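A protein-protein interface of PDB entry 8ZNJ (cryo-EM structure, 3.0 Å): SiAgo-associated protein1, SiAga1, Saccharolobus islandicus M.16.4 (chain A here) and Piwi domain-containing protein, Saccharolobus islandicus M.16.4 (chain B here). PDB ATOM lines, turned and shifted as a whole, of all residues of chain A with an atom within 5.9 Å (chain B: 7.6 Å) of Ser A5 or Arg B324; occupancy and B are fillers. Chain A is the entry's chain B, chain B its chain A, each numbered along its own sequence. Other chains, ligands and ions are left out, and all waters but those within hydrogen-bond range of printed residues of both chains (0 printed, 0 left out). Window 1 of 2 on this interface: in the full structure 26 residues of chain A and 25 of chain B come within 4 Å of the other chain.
The side-chain carboxylate (OD2) of Asp A169 sits close to the backbone carbonyl oxygen (O) of Pro B322 (3.4 Å).
N of Phe B326 is in hydrogen-bond range of O of Glu A4, 2.9 Å away.
The guanidinium group (NE) of Arg A200 sits at hydrogen-bond distance from the side-chain hydroxyl (OG1) of Thr B387.
O of Pro B322 lies within hydrogen-bond range of ND2 of Asn A6 (3.1 Å).
O of Arg B324 sits at hydrogen-bond distance from N of Asn A6, 3.2 Å away.
The guanidinium group (NE) of Arg B324 is in salt-bridge range of the side-chain carboxylate (OD2) of Asp A169, 3.1 Å away.
The guanidinium group of Arg B324 sits at hydrogen-bond distance from the backbone carbonyl oxygen of Pro B388, 2.7 Å away.
The side-chain hydroxyl (OG) of Ser A5 is in hydrogen-bond range of the side-chain hydroxyl (OG1) of Thr A233.
The backbone carbonyl oxygen (O) of Met A7 lies within hydrogen-bond range of the backbone NH (N) of Thr A233 (3.5 Å).
NH1 of Arg B324 sits at hydrogen-bond distance from O of Thr B387.
The side-chain carboxylate of Asp A169 is in salt-bridge range of the side-chain amino group of Lys A171, at 3.95 Å.
The side-chain sulfur (SD) of Met A7 lies within hydrogen-bond range of the side-chain hydroxyl (OH) of Tyr A167 (3.2 Å).
Among the printed residues, pairs that only touch across the chains: Leu A3 with Phe B326, Leu A3 with Ile B325, Ser A5 with Arg B324, Tyr A201 with Phe B326, Tyr A167 with Pro B322, Tyr A167 with Val B323, Glu A4 with Gly B327, Leu A3 with Gly B327, Asn A6 with Val B323, Leu A3 with Val B335, Met A7 with Glu B3 and Glu A4 with Ile B325.
Of chain B, only Arg B324 comes within 4 Å of Ser A5.
Arg B324 touches three residues of chain A.
Of the printed residues of chain A, Gly B327 touches Leu A3 and Glu A4.
Printed residues of chain A within 4 Å of Ile B325: Leu A3 and Glu A4.
The nearest printed residue of chain B that does not touch Tyr A201 is Gly B327 (5.9 Å).
Of the 14 printed residues of chain A, 9 touch a printed residue of chain B.
Of the 17 printed residues of chain B, 9 touch a printed residue of chain A.
Hydrophobic or aromatic side chains of chain B within 4 Å of the printed part of chain A: Pro B322, Val B323, Ile B325, Phe B326 and Val B335.
Among the printed residues, Asp or Glu carboxylates within 4 Å of a Lys or Arg side-chain nitrogen of the other chain: Asp A169 with Arg B324.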
ATOM      1  N   LEU A   3      22.887 -16.843   2.673  1.00  0.00           N
ATOM      2  CA  LEU A   3      22.731 -15.645   3.498  1.00  0.00           C
ATOM      3  C   LEU A   3      21.410 -15.665   4.266  1.00  0.00           C
ATOM      4  O   LEU A   3      20.675 -14.677   4.317  1.00  0.00           O
ATOM      5  CB  LEU A   3      22.854 -14.382   2.644  1.00  0.00           C
ATOM      6  CG  LEU A   3      24.202 -13.666   2.741  1.00  0.00           C
ATOM      7  CD1 LEU A   3      24.360 -13.029   4.110  1.00  0.00           C
ATOM      8  CD2 LEU A   3      25.349 -14.621   2.455  1.00  0.00           C
ATOM      9  N   GLU A   4      21.106 -16.806   4.874  1.00  0.00           N
ATOM     10  CA  GLU A   4      19.921 -16.912   5.711  1.00  0.00           C
ATOM     11  C   GLU A   4      20.073 -16.015   6.935  1.00  0.00           C
ATOM     12  O   GLU A   4      21.176 -15.804   7.443  1.00  0.00           O
ATOM     13  CB  GLU A   4      19.708 -18.369   6.125  1.00  0.00           C
ATOM     14  CG  GLU A   4      19.133 -18.583   7.513  1.00  0.00           C
ATOM     15  CD  GLU A   4      18.529 -19.964   7.667  1.00  0.00           C
ATOM     16  OE1 GLU A   4      19.252 -20.952   7.423  1.00  0.00           O
ATOM     17  OE2 GLU A   4      17.337 -20.066   8.024  1.00  0.00           O
ATOM     18  N   SER A   5      18.953 -15.479   7.408  1.00  0.00           N
ATOM     19  CA  SER A   5      18.942 -14.538   8.520  1.00  0.00           C
ATOM     20  C   SER A   5      18.022 -15.052   9.629  1.00  0.00           C
ATOM     21  O   SER A   5      17.524 -16.179   9.583  1.00  0.00           O
ATOM     22  CB  SER A   5      18.512 -13.153   8.038  1.00  0.00           C
ATOM     23  OG  SER A   5      17.135 -13.134   7.715  1.00  0.00           O
ATOM     24  N   ASN A   6      17.812 -14.211  10.639  1.00  0.00           N
ATOM     25  CA  ASN A   6      16.953 -14.535  11.766  1.00  0.00           C
ATOM     26  C   ASN A   6      15.594 -13.857  11.692  1.00  0.00           C
ATOM     27  O   ASN A   6      14.810 -13.970  12.636  1.00  0.00           O
ATOM     28  CB  ASN A   6      17.645 -14.156  13.081  1.00  0.00           C
ATOM     29  CG  ASN A   6      17.606 -12.664  13.362  1.00  0.00           C
ATOM     30  OD1 ASN A   6      17.243 -11.863  12.504  1.00  0.00           O
ATOM     31  ND2 ASN A   6      17.986 -12.285  14.574  1.00  0.00           N
ATOM     32  N   MET A   7      15.296 -13.161  10.599  1.00  0.00           N
ATOM     33  CA  MET A   7      14.068 -12.391  10.470  1.00  0.00           C
ATOM     34  C   MET A   7      13.008 -13.193   9.733  1.00  0.00           C
ATOM     35  O   MET A   7      13.274 -13.757   8.667  1.00  0.00           O
ATOM     36  CB  MET A   7      14.321 -11.077   9.731  1.00  0.00           C
ATOM     37  CG  MET A   7      13.162 -10.092   9.832  1.00  0.00           C
ATOM     38  SD  MET A   7      13.152  -8.805   8.564  1.00  0.00           S
ATOM     39  CE  MET A   7      13.355  -9.761   7.064  1.00  0.00           C
ATOM     40  N   TYR A 167      11.874 -10.612  14.699  1.00  0.00           N
ATOM     41  CA  TYR A 167      13.277 -10.935  14.910  1.00  0.00           C
ATOM     42  C   TYR A 167      13.399 -11.747  16.189  1.00  0.00           C
ATOM     43  O   TYR A 167      12.976 -11.292  17.256  1.00  0.00           O
ATOM     44  CB  TYR A 167      14.124  -9.668  15.015  1.00  0.00           C
ATOM     45  CG  TYR A 167      14.085  -8.778  13.796  1.00  0.00           C
ATOM     46  CD1 TYR A 167      13.142  -7.765  13.681  1.00  0.00           C
ATOM     47  CD2 TYR A 167      15.007  -8.933  12.773  1.00  0.00           C
ATOM     48  CE1 TYR A 167      13.112  -6.945  12.571  1.00  0.00           C
ATOM     49  CE2 TYR A 167      14.988  -8.115  11.665  1.00  0.00           C
ATOM     50  CZ  TYR A 167      14.036  -7.124  11.566  1.00  0.00           C
ATOM     51  OH  TYR A 167      14.012  -6.309  10.459  1.00  0.00           O
ATOM     52  N   ASP A 169      16.325 -13.569  18.526  1.00  0.00           N
ATOM     53  CA  ASP A 169      17.765 -13.614  18.742  1.00  0.00           C
ATOM     54  C   ASP A 169      18.053 -14.227  20.103  1.00  0.00           C
ATOM     55  O   ASP A 169      17.163 -14.393  20.936  1.00  0.00           O
ATOM     56  CB  ASP A 169      18.396 -12.223  18.630  1.00  0.00           C
ATOM     57  CG  ASP A 169      19.770 -12.254  17.977  1.00  0.00           C
ATOM     58  OD1 ASP A 169      20.323 -13.358  17.783  1.00  0.00           O
ATOM     59  OD2 ASP A 169      20.300 -11.169  17.654  1.00  0.00           O
ATOM     60  N   LYS A 171      19.721 -14.176  23.712  1.00  0.00           N
ATOM     61  CA  LYS A 171      20.115 -13.205  24.721  1.00  0.00           C
ATOM     62  C   LYS A 171      20.251 -13.883  26.076  1.00  0.00           C
ATOM     63  O   LYS A 171      19.516 -14.818  26.402  1.00  0.00           O
ATOM     64  CB  LYS A 171      19.108 -12.052  24.826  1.00  0.00           C
ATOM     65  CG  LYS A 171      18.842 -11.327  23.515  1.00  0.00           C
ATOM     66  CD  LYS A 171      20.040 -10.498  23.077  1.00  0.00           C
ATOM     67  CE  LYS A 171      19.807  -9.859  21.717  1.00  0.00           C
ATOM     68  NZ  LYS A 171      21.074  -9.382  21.095  1.00  0.00           N
ATOM     69  N   ARG A 200      24.668 -19.855  17.991  1.00  0.00           N
ATOM     70  CA  ARG A 200      23.546 -18.925  17.912  1.00  0.00           C
ATOM     71  C   ARG A 200      22.540 -19.359  16.853  1.00  0.00           C
ATOM     72  O   ARG A 200      21.327 -19.343  17.089  1.00  0.00           O
ATOM     73  CB  ARG A 200      24.068 -17.522  17.613  1.00  0.00           C
ATOM     74  CG  ARG A 200      23.084 -16.409  17.892  1.00  0.00           C
ATOM     75  CD  ARG A 200      23.753 -15.057  17.761  1.00  0.00           C
ATOM     76  NE  ARG A 200      24.832 -14.891  18.728  1.00  0.00           N
ATOM     77  CZ  ARG A 200      24.734 -14.217  19.864  1.00  0.00           C
ATOM     78  NH1 ARG A 200      23.611 -13.616  20.222  1.00  0.00           N
ATOM     79  NH2 ARG A 200      25.792 -14.142  20.666  1.00  0.00           N
ATOM     80  N   TYR A 201      23.026 -19.742  15.671  1.00  0.00           N
ATOM     81  CA  TYR A 201      22.118 -20.142  14.600  1.00  0.00           C
ATOM     82  C   TYR A 201      21.344 -21.399  14.975  1.00  0.00           C
ATOM     83  O   TYR A 201      20.129 -21.478  14.758  1.00  0.00           O
ATOM     84  CB  TYR A 201      22.905 -20.351  13.308  1.00  0.00           C
ATOM     85  CG  TYR A 201      22.117 -20.994  12.191  1.00  0.00           C
ATOM     86  CD1 TYR A 201      21.995 -22.374  12.107  1.00  0.00           C
ATOM     87  CD2 TYR A 201      21.500 -20.222  11.219  1.00  0.00           C
ATOM     88  CE1 TYR A 201      21.283 -22.966  11.090  1.00  0.00           C
ATOM     89  CE2 TYR A 201      20.783 -20.807  10.195  1.00  0.00           C
ATOM     90  CZ  TYR A 201      20.678 -22.181  10.138  1.00  0.00           C
ATOM     91  OH  TYR A 201      19.967 -22.778   9.124  1.00  0.00           O
ATOM     92  N   ILE A 204      18.705 -20.512  17.567  1.00  0.00           N
ATOM     93  CA  ILE A 204      17.531 -19.904  16.947  1.00  0.00           C
ATOM     94  C   ILE A 204      16.695 -20.966  16.245  1.00  0.00           C
ATOM     95  O   ILE A 204      15.459 -20.966  16.329  1.00  0.00           O
ATOM     96  CB  ILE A 204      17.963 -18.788  15.977  1.00  0.00           C
ATOM     97  CG1 ILE A 204      18.277 -17.505  16.749  1.00  0.00           C
ATOM     98  CG2 ILE A 204      16.884 -18.532  14.932  1.00  0.00           C
ATOM     99  CD1 ILE A 204      18.998 -16.454  15.924  1.00  0.00           C
ATOM    100  N   ARG A 232      10.977 -17.085   6.911  1.00  0.00           N
ATOM    101  CA  ARG A 232      12.358 -16.640   7.003  1.00  0.00           C
ATOM    102  C   ARG A 232      12.872 -16.267   5.618  1.00  0.00           C
ATOM    103  O   ARG A 232      12.507 -16.878   4.609  1.00  0.00           O
ATOM    104  CB  ARG A 232      13.234 -17.727   7.627  1.00  0.00           C
ATOM    105  CG  ARG A 232      14.438 -17.186   8.389  1.00  0.00           C
ATOM    106  CD  ARG A 232      15.288 -18.303   8.977  1.00  0.00           C
ATOM    107  NE  ARG A 232      14.853 -18.677  10.318  1.00  0.00           N
ATOM    108  CZ  ARG A 232      15.601 -19.325  11.202  1.00  0.00           C
ATOM    109  NH1 ARG A 232      16.853 -19.662  10.938  1.00  0.00           N
ATOM    110  NH2 ARG A 232      15.081 -19.640  12.386  1.00  0.00           N
ATOM    111  N   THR A 233      13.729 -15.250   5.575  1.00  0.00           N
ATOM    112  CA  THR A 233      14.098 -14.618   4.313  1.00  0.00           C
ATOM    113  C   THR A 233      14.763 -15.594   3.350  1.00  0.00           C
ATOM    114  O   THR A 233      14.204 -15.905   2.293  1.00  0.00           O
ATOM    115  CB  THR A 233      15.031 -13.436   4.573  1.00  0.00           C
ATOM    116  OG1 THR A 233      16.104 -13.851   5.426  1.00  0.00           O
ATOM    117  CG2 THR A 233      14.274 -12.300   5.239  1.00  0.00           C
ATOM    118  N   LYS A 234      15.944 -16.090   3.706  1.00  0.00           N
ATOM    119  CA  LYS A 234      16.729 -16.958   2.830  1.00  0.00           C
ATOM    120  C   LYS A 234      16.886 -16.332   1.443  1.00  0.00           C
ATOM    121  O   LYS A 234      16.523 -16.913   0.419  1.00  0.00           O
ATOM    122  CB  LYS A 234      16.101 -18.350   2.739  1.00  0.00           C
ATOM    123  CG  LYS A 234      16.054 -19.089   4.063  1.00  0.00           C
ATOM    124  CD  LYS A 234      15.781 -20.567   3.858  1.00  0.00           C
ATOM    125  CE  LYS A 234      15.802 -21.323   5.175  1.00  0.00           C
ATOM    126  NZ  LYS A 234      15.784 -22.796   4.968  1.00  0.00           N
ATOM    127  N   GLU B   3      12.706  -7.163  -1.525  1.00  0.00           N
ATOM    128  CA  GLU B   3      13.839  -7.346  -0.628  1.00  0.00           C
ATOM    129  C   GLU B   3      14.876  -8.220  -1.321  1.00  0.00           C
ATOM    130  O   GLU B   3      14.572  -9.346  -1.728  1.00  0.00           O
ATOM    131  CB  GLU B   3      13.394  -7.984   0.688  1.00  0.00           C
ATOM    132  CG  GLU B   3      14.531  -8.585   1.503  1.00  0.00           C
ATOM    133  CD  GLU B   3      14.274  -8.538   2.997  1.00  0.00           C
ATOM    134  OE1 GLU B   3      13.097  -8.416   3.397  1.00  0.00           O
ATOM    135  OE2 GLU B   3      15.248  -8.623   3.772  1.00  0.00           O
ATOM    136  N   THR B 321      20.290  -3.059  16.943  1.00  0.00           N
ATOM    137  CA  THR B 321      19.282  -3.686  16.107  1.00  0.00           C
ATOM    138  C   THR B 321      19.208  -5.172  16.418  1.00  0.00           C
ATOM    139  O   THR B 321      20.190  -5.763  16.876  1.00  0.00           O
ATOM    140  CB  THR B 321      19.594  -3.490  14.615  1.00  0.00           C
ATOM    141  OG1 THR B 321      18.839  -4.423  13.836  1.00  0.00           O
ATOM    142  CG2 THR B 321      21.072  -3.688  14.343  1.00  0.00           C
ATOM    143  N   PRO B 322      18.050  -5.802  16.193  1.00  0.00           N
ATOM    144  CA  PRO B 322      17.927  -7.241  16.450  1.00  0.00           C
ATOM    145  C   PRO B 322      18.310  -8.133  15.281  1.00  0.00           C
ATOM    146  O   PRO B 322      18.439  -9.349  15.476  1.00  0.00           O
ATOM    147  CB  PRO B 322      16.434  -7.392  16.775  1.00  0.00           C
ATOM    148  CG  PRO B 322      15.775  -6.324  15.985  1.00  0.00           C
ATOM    149  CD  PRO B 322      16.749  -5.185  15.880  1.00  0.00           C
ATOM    150  N   VAL B 323      18.504  -7.573  14.088  1.00  0.00           N
ATOM    151  CA  VAL B 323      18.748  -8.387  12.903  1.00  0.00           C
ATOM    152  C   VAL B 323      20.108  -9.066  13.010  1.00  0.00           C
ATOM    153  O   VAL B 323      21.107  -8.444  13.393  1.00  0.00           O
ATOM    154  CB  VAL B 323      18.654  -7.528  11.633  1.00  0.00           C
ATOM    155  CG1 VAL B 323      19.776  -6.509  11.590  1.00  0.00           C
ATOM    156  CG2 VAL B 323      18.682  -8.406  10.395  1.00  0.00           C
ATOM    157  N   ARG B 324      20.143 -10.356  12.679  1.00  0.00           N
ATOM    158  CA  ARG B 324      21.374 -11.119  12.551  1.00  0.00           C
ATOM    159  C   ARG B 324      21.385 -11.790  11.188  1.00  0.00           C
ATOM    160  O   ARG B 324      20.339 -12.187  10.671  1.00  0.00           O
ATOM    161  CB  ARG B 324      21.508 -12.182  13.646  1.00  0.00           C
ATOM    162  CG  ARG B 324      21.652 -11.628  15.049  1.00  0.00           C
ATOM    163  CD  ARG B 324      23.085 -11.241  15.356  1.00  0.00           C
ATOM    164  NE  ARG B 324      23.204 -10.624  16.670  1.00  0.00           N
ATOM    165  CZ  ARG B 324      24.354 -10.344  17.267  1.00  0.00           C
ATOM    166  NH1 ARG B 324      25.512 -10.614  16.694  1.00  0.00           N
ATOM    167  NH2 ARG B 324      24.339  -9.783  18.470  1.00  0.00           N
ATOM    168  N   ILE B 325      22.575 -11.913  10.609  1.00  0.00           N
ATOM    169  CA  ILE B 325      22.740 -12.480   9.277  1.00  0.00           C
ATOM    170  C   ILE B 325      23.798 -13.570   9.346  1.00  0.00           C
ATOM    171  O   ILE B 325      24.948 -13.305   9.716  1.00  0.00           O
ATOM    172  CB  ILE B 325      23.128 -11.416   8.238  1.00  0.00           C
ATOM    173  CG1 ILE B 325      22.233 -10.184   8.370  1.00  0.00           C
ATOM    174  CG2 ILE B 325      23.019 -11.982   6.836  1.00  0.00           C
ATOM    175  CD1 ILE B 325      22.694  -9.012   7.544  1.00  0.00           C
ATOM    176  N   PHE B 326      23.408 -14.790   9.002  1.00  0.00           N
ATOM    177  CA  PHE B 326      24.301 -15.926   8.830  1.00  0.00           C
ATOM    178  C   PHE B 326      24.167 -16.411   7.387  1.00  0.00           C
ATOM    179  O   PHE B 326      23.542 -15.751   6.554  1.00  0.00           O
ATOM    180  CB  PHE B 326      23.962 -17.038   9.825  1.00  0.00           C
ATOM    181  CG  PHE B 326      23.296 -16.555  11.080  1.00  0.00           C
ATOM    182  CD1 PHE B 326      24.042 -16.074  12.139  1.00  0.00           C
ATOM    183  CD2 PHE B 326      21.918 -16.595  11.202  1.00  0.00           C
ATOM    184  CE1 PHE B 326      23.426 -15.636  13.293  1.00  0.00           C
ATOM    185  CE2 PHE B 326      21.300 -16.158  12.352  1.00  0.00           C
ATOM    186  CZ  PHE B 326      22.056 -15.679  13.398  1.00  0.00           C
ATOM    187  N   GLY B 327      24.757 -17.555   7.084  1.00  0.00           N
ATOM    188  CA  GLY B 327      24.387 -18.257   5.871  1.00  0.00           C
ATOM    189  C   GLY B 327      25.524 -19.066   5.282  1.00  0.00           C
ATOM    190  O   GLY B 327      26.616 -19.163   5.834  1.00  0.00           O
ATOM    191  N   VAL B 335      29.470 -14.803   8.077  1.00  0.00           N
ATOM    192  CA  VAL B 335      28.970 -13.946   7.010  1.00  0.00           C
ATOM    193  C   VAL B 335      30.079 -12.994   6.590  1.00  0.00           C
ATOM    194  O   VAL B 335      30.765 -12.418   7.441  1.00  0.00           O
ATOM    195  CB  VAL B 335      27.717 -13.167   7.451  1.00  0.00           C
ATOM    196  CG1 VAL B 335      27.922 -12.556   8.826  1.00  0.00           C
ATOM    197  CG2 VAL B 335      27.368 -12.095   6.430  1.00  0.00           C
ATOM    198  N   ILE B 341      21.703  -5.997   2.838  1.00  0.00           N
ATOM    199  CA  ILE B 341      20.328  -6.441   2.638  1.00  0.00           C
ATOM    200  C   ILE B 341      19.500  -5.189   2.382  1.00  0.00           C
ATOM    201  O   ILE B 341      19.358  -4.342   3.272  1.00  0.00           O
ATOM    202  CB  ILE B 341      19.786  -7.209   3.852  1.00  0.00           C
ATOM    203  CG1 ILE B 341      20.834  -8.174   4.416  1.00  0.00           C
ATOM    204  CG2 ILE B 341      18.510  -7.950   3.482  1.00  0.00           C
ATOM    205  CD1 ILE B 341      21.268  -9.251   3.462  1.00  0.00           C
ATOM    206  N   VAL B 361      20.375  -3.001   5.615  1.00  0.00           N
ATOM    207  CA  VAL B 361      21.086  -3.625   6.724  1.00  0.00           C
ATOM    208  C   VAL B 361      22.462  -4.037   6.222  1.00  0.00           C
ATOM    209  O   VAL B 361      22.578  -4.887   5.334  1.00  0.00           O
ATOM    210  CB  VAL B 361      20.317  -4.835   7.276  1.00  0.00           C
ATOM    211  CG1 VAL B 361      21.137  -5.542   8.339  1.00  0.00           C
ATOM    212  CG2 VAL B 361      18.976  -4.399   7.836  1.00  0.00           C
ATOM    213  N   THR B 363      26.368  -5.381   7.224  1.00  0.00           N
ATOM    214  CA  THR B 363      27.353  -5.916   8.150  1.00  0.00           C
ATOM    215  C   THR B 363      28.684  -5.232   7.871  1.00  0.00           C
ATOM    216  O   THR B 363      29.104  -5.129   6.716  1.00  0.00           O
ATOM    217  CB  THR B 363      27.489  -7.433   8.001  1.00  0.00           C
ATOM    218  OG1 THR B 363      26.198  -8.047   8.105  1.00  0.00           O
ATOM    219  CG2 THR B 363      28.396  -7.995   9.080  1.00  0.00           C
ATOM    220  N   GLY B 386      32.793 -13.818  18.182  1.00  0.00           N
ATOM    221  CA  GLY B 386      31.395 -13.511  18.410  1.00  0.00           C
ATOM    222  C   GLY B 386      30.587 -13.585  17.134  1.00  0.00           C
ATOM    223  O   GLY B 386      30.944 -14.322  16.210  1.00  0.00           O
ATOM    224  N   THR B 387      29.495 -12.825  17.068  1.00  0.00           N
ATOM    225  CA  THR B 387      28.660 -12.765  15.885  1.00  0.00           C
ATOM    226  C   THR B 387      28.500 -11.317  15.433  1.00  0.00           C
ATOM    227  O   THR B 387      28.339 -10.429  16.274  1.00  0.00           O
ATOM    228  CB  THR B 387      27.277 -13.370  16.155  1.00  0.00           C
ATOM    229  OG1 THR B 387      27.429 -14.683  16.708  1.00  0.00           O
ATOM    230  CG2 THR B 387      26.466 -13.453  14.873  1.00  0.00           C
ATOM    231  N   PRO B 388      28.533 -11.045  14.127  1.00  0.00           N
ATOM    232  CA  PRO B 388      28.422  -9.657  13.665  1.00  0.00           C
ATOM    233  C   PRO B 388      27.141  -8.985  14.139  1.00  0.00           C
ATOM    234  O   PRO B 388      26.078  -9.604  14.205  1.00  0.00           O
ATOM    235  CB  PRO B 388      28.445  -9.795  12.142  1.00  0.00           C
ATOM    236  CG  PRO B 388      29.239 -11.008  11.900  1.00  0.00           C
ATOM    237  CD  PRO B 388      28.902 -11.949  13.021  1.00  0.00           C
ATOM    238  N   ARG B 389      27.259  -7.696  14.457  1.00  0.00           N
ATOM    239  CA  ARG B 389      26.131  -6.836  14.800  1.00  0.00           C
ATOM    240  C   ARG B 389      25.937  -5.845  13.661  1.00  0.00           C
ATOM    241  O   ARG B 389      26.522  -4.753  13.675  1.00  0.00           O
ATOM    242  CB  ARG B 389      26.375  -6.098  16.117  1.00  0.00           C
ATOM    243  CG  ARG B 389      26.736  -6.990  17.281  1.00  0.00           C
ATOM    244  CD  ARG B 389      26.662  -6.230  18.592  1.00  0.00           C
ATOM    245  NE  ARG B 389      27.517  -5.048  18.597  1.00  0.00           N
ATOM    246  CZ  ARG B 389      27.719  -4.277  19.657  1.00  0.00           C
ATOM    247  NH1 ARG B 389      27.144  -4.535  20.819  1.00  0.00           N
ATOM    248  NH2 ARG B 389      28.518  -3.220  19.548  1.00  0.00           N
ATOM    249  N   PRO B 390      25.134  -6.169  12.650  1.00  0.00           N
ATOM    250  CA  PRO B 390      24.960  -5.240  11.533  1.00  0.00           C
ATOM    251  C   PRO B 390      24.297  -3.946  11.978  1.00  0.00           C
ATOM    252  O   PRO B 390      23.672  -3.862  13.035  1.00  0.00           O
ATOM    253  CB  PRO B 390      24.068  -6.014  10.554  1.00  0.00           C
ATOM    254  CG  PRO B 390      23.463  -7.104  11.351  1.00  0.00           C
ATOM    255  CD  PRO B 390      24.442  -7.446  12.415  1.00  0.00           C
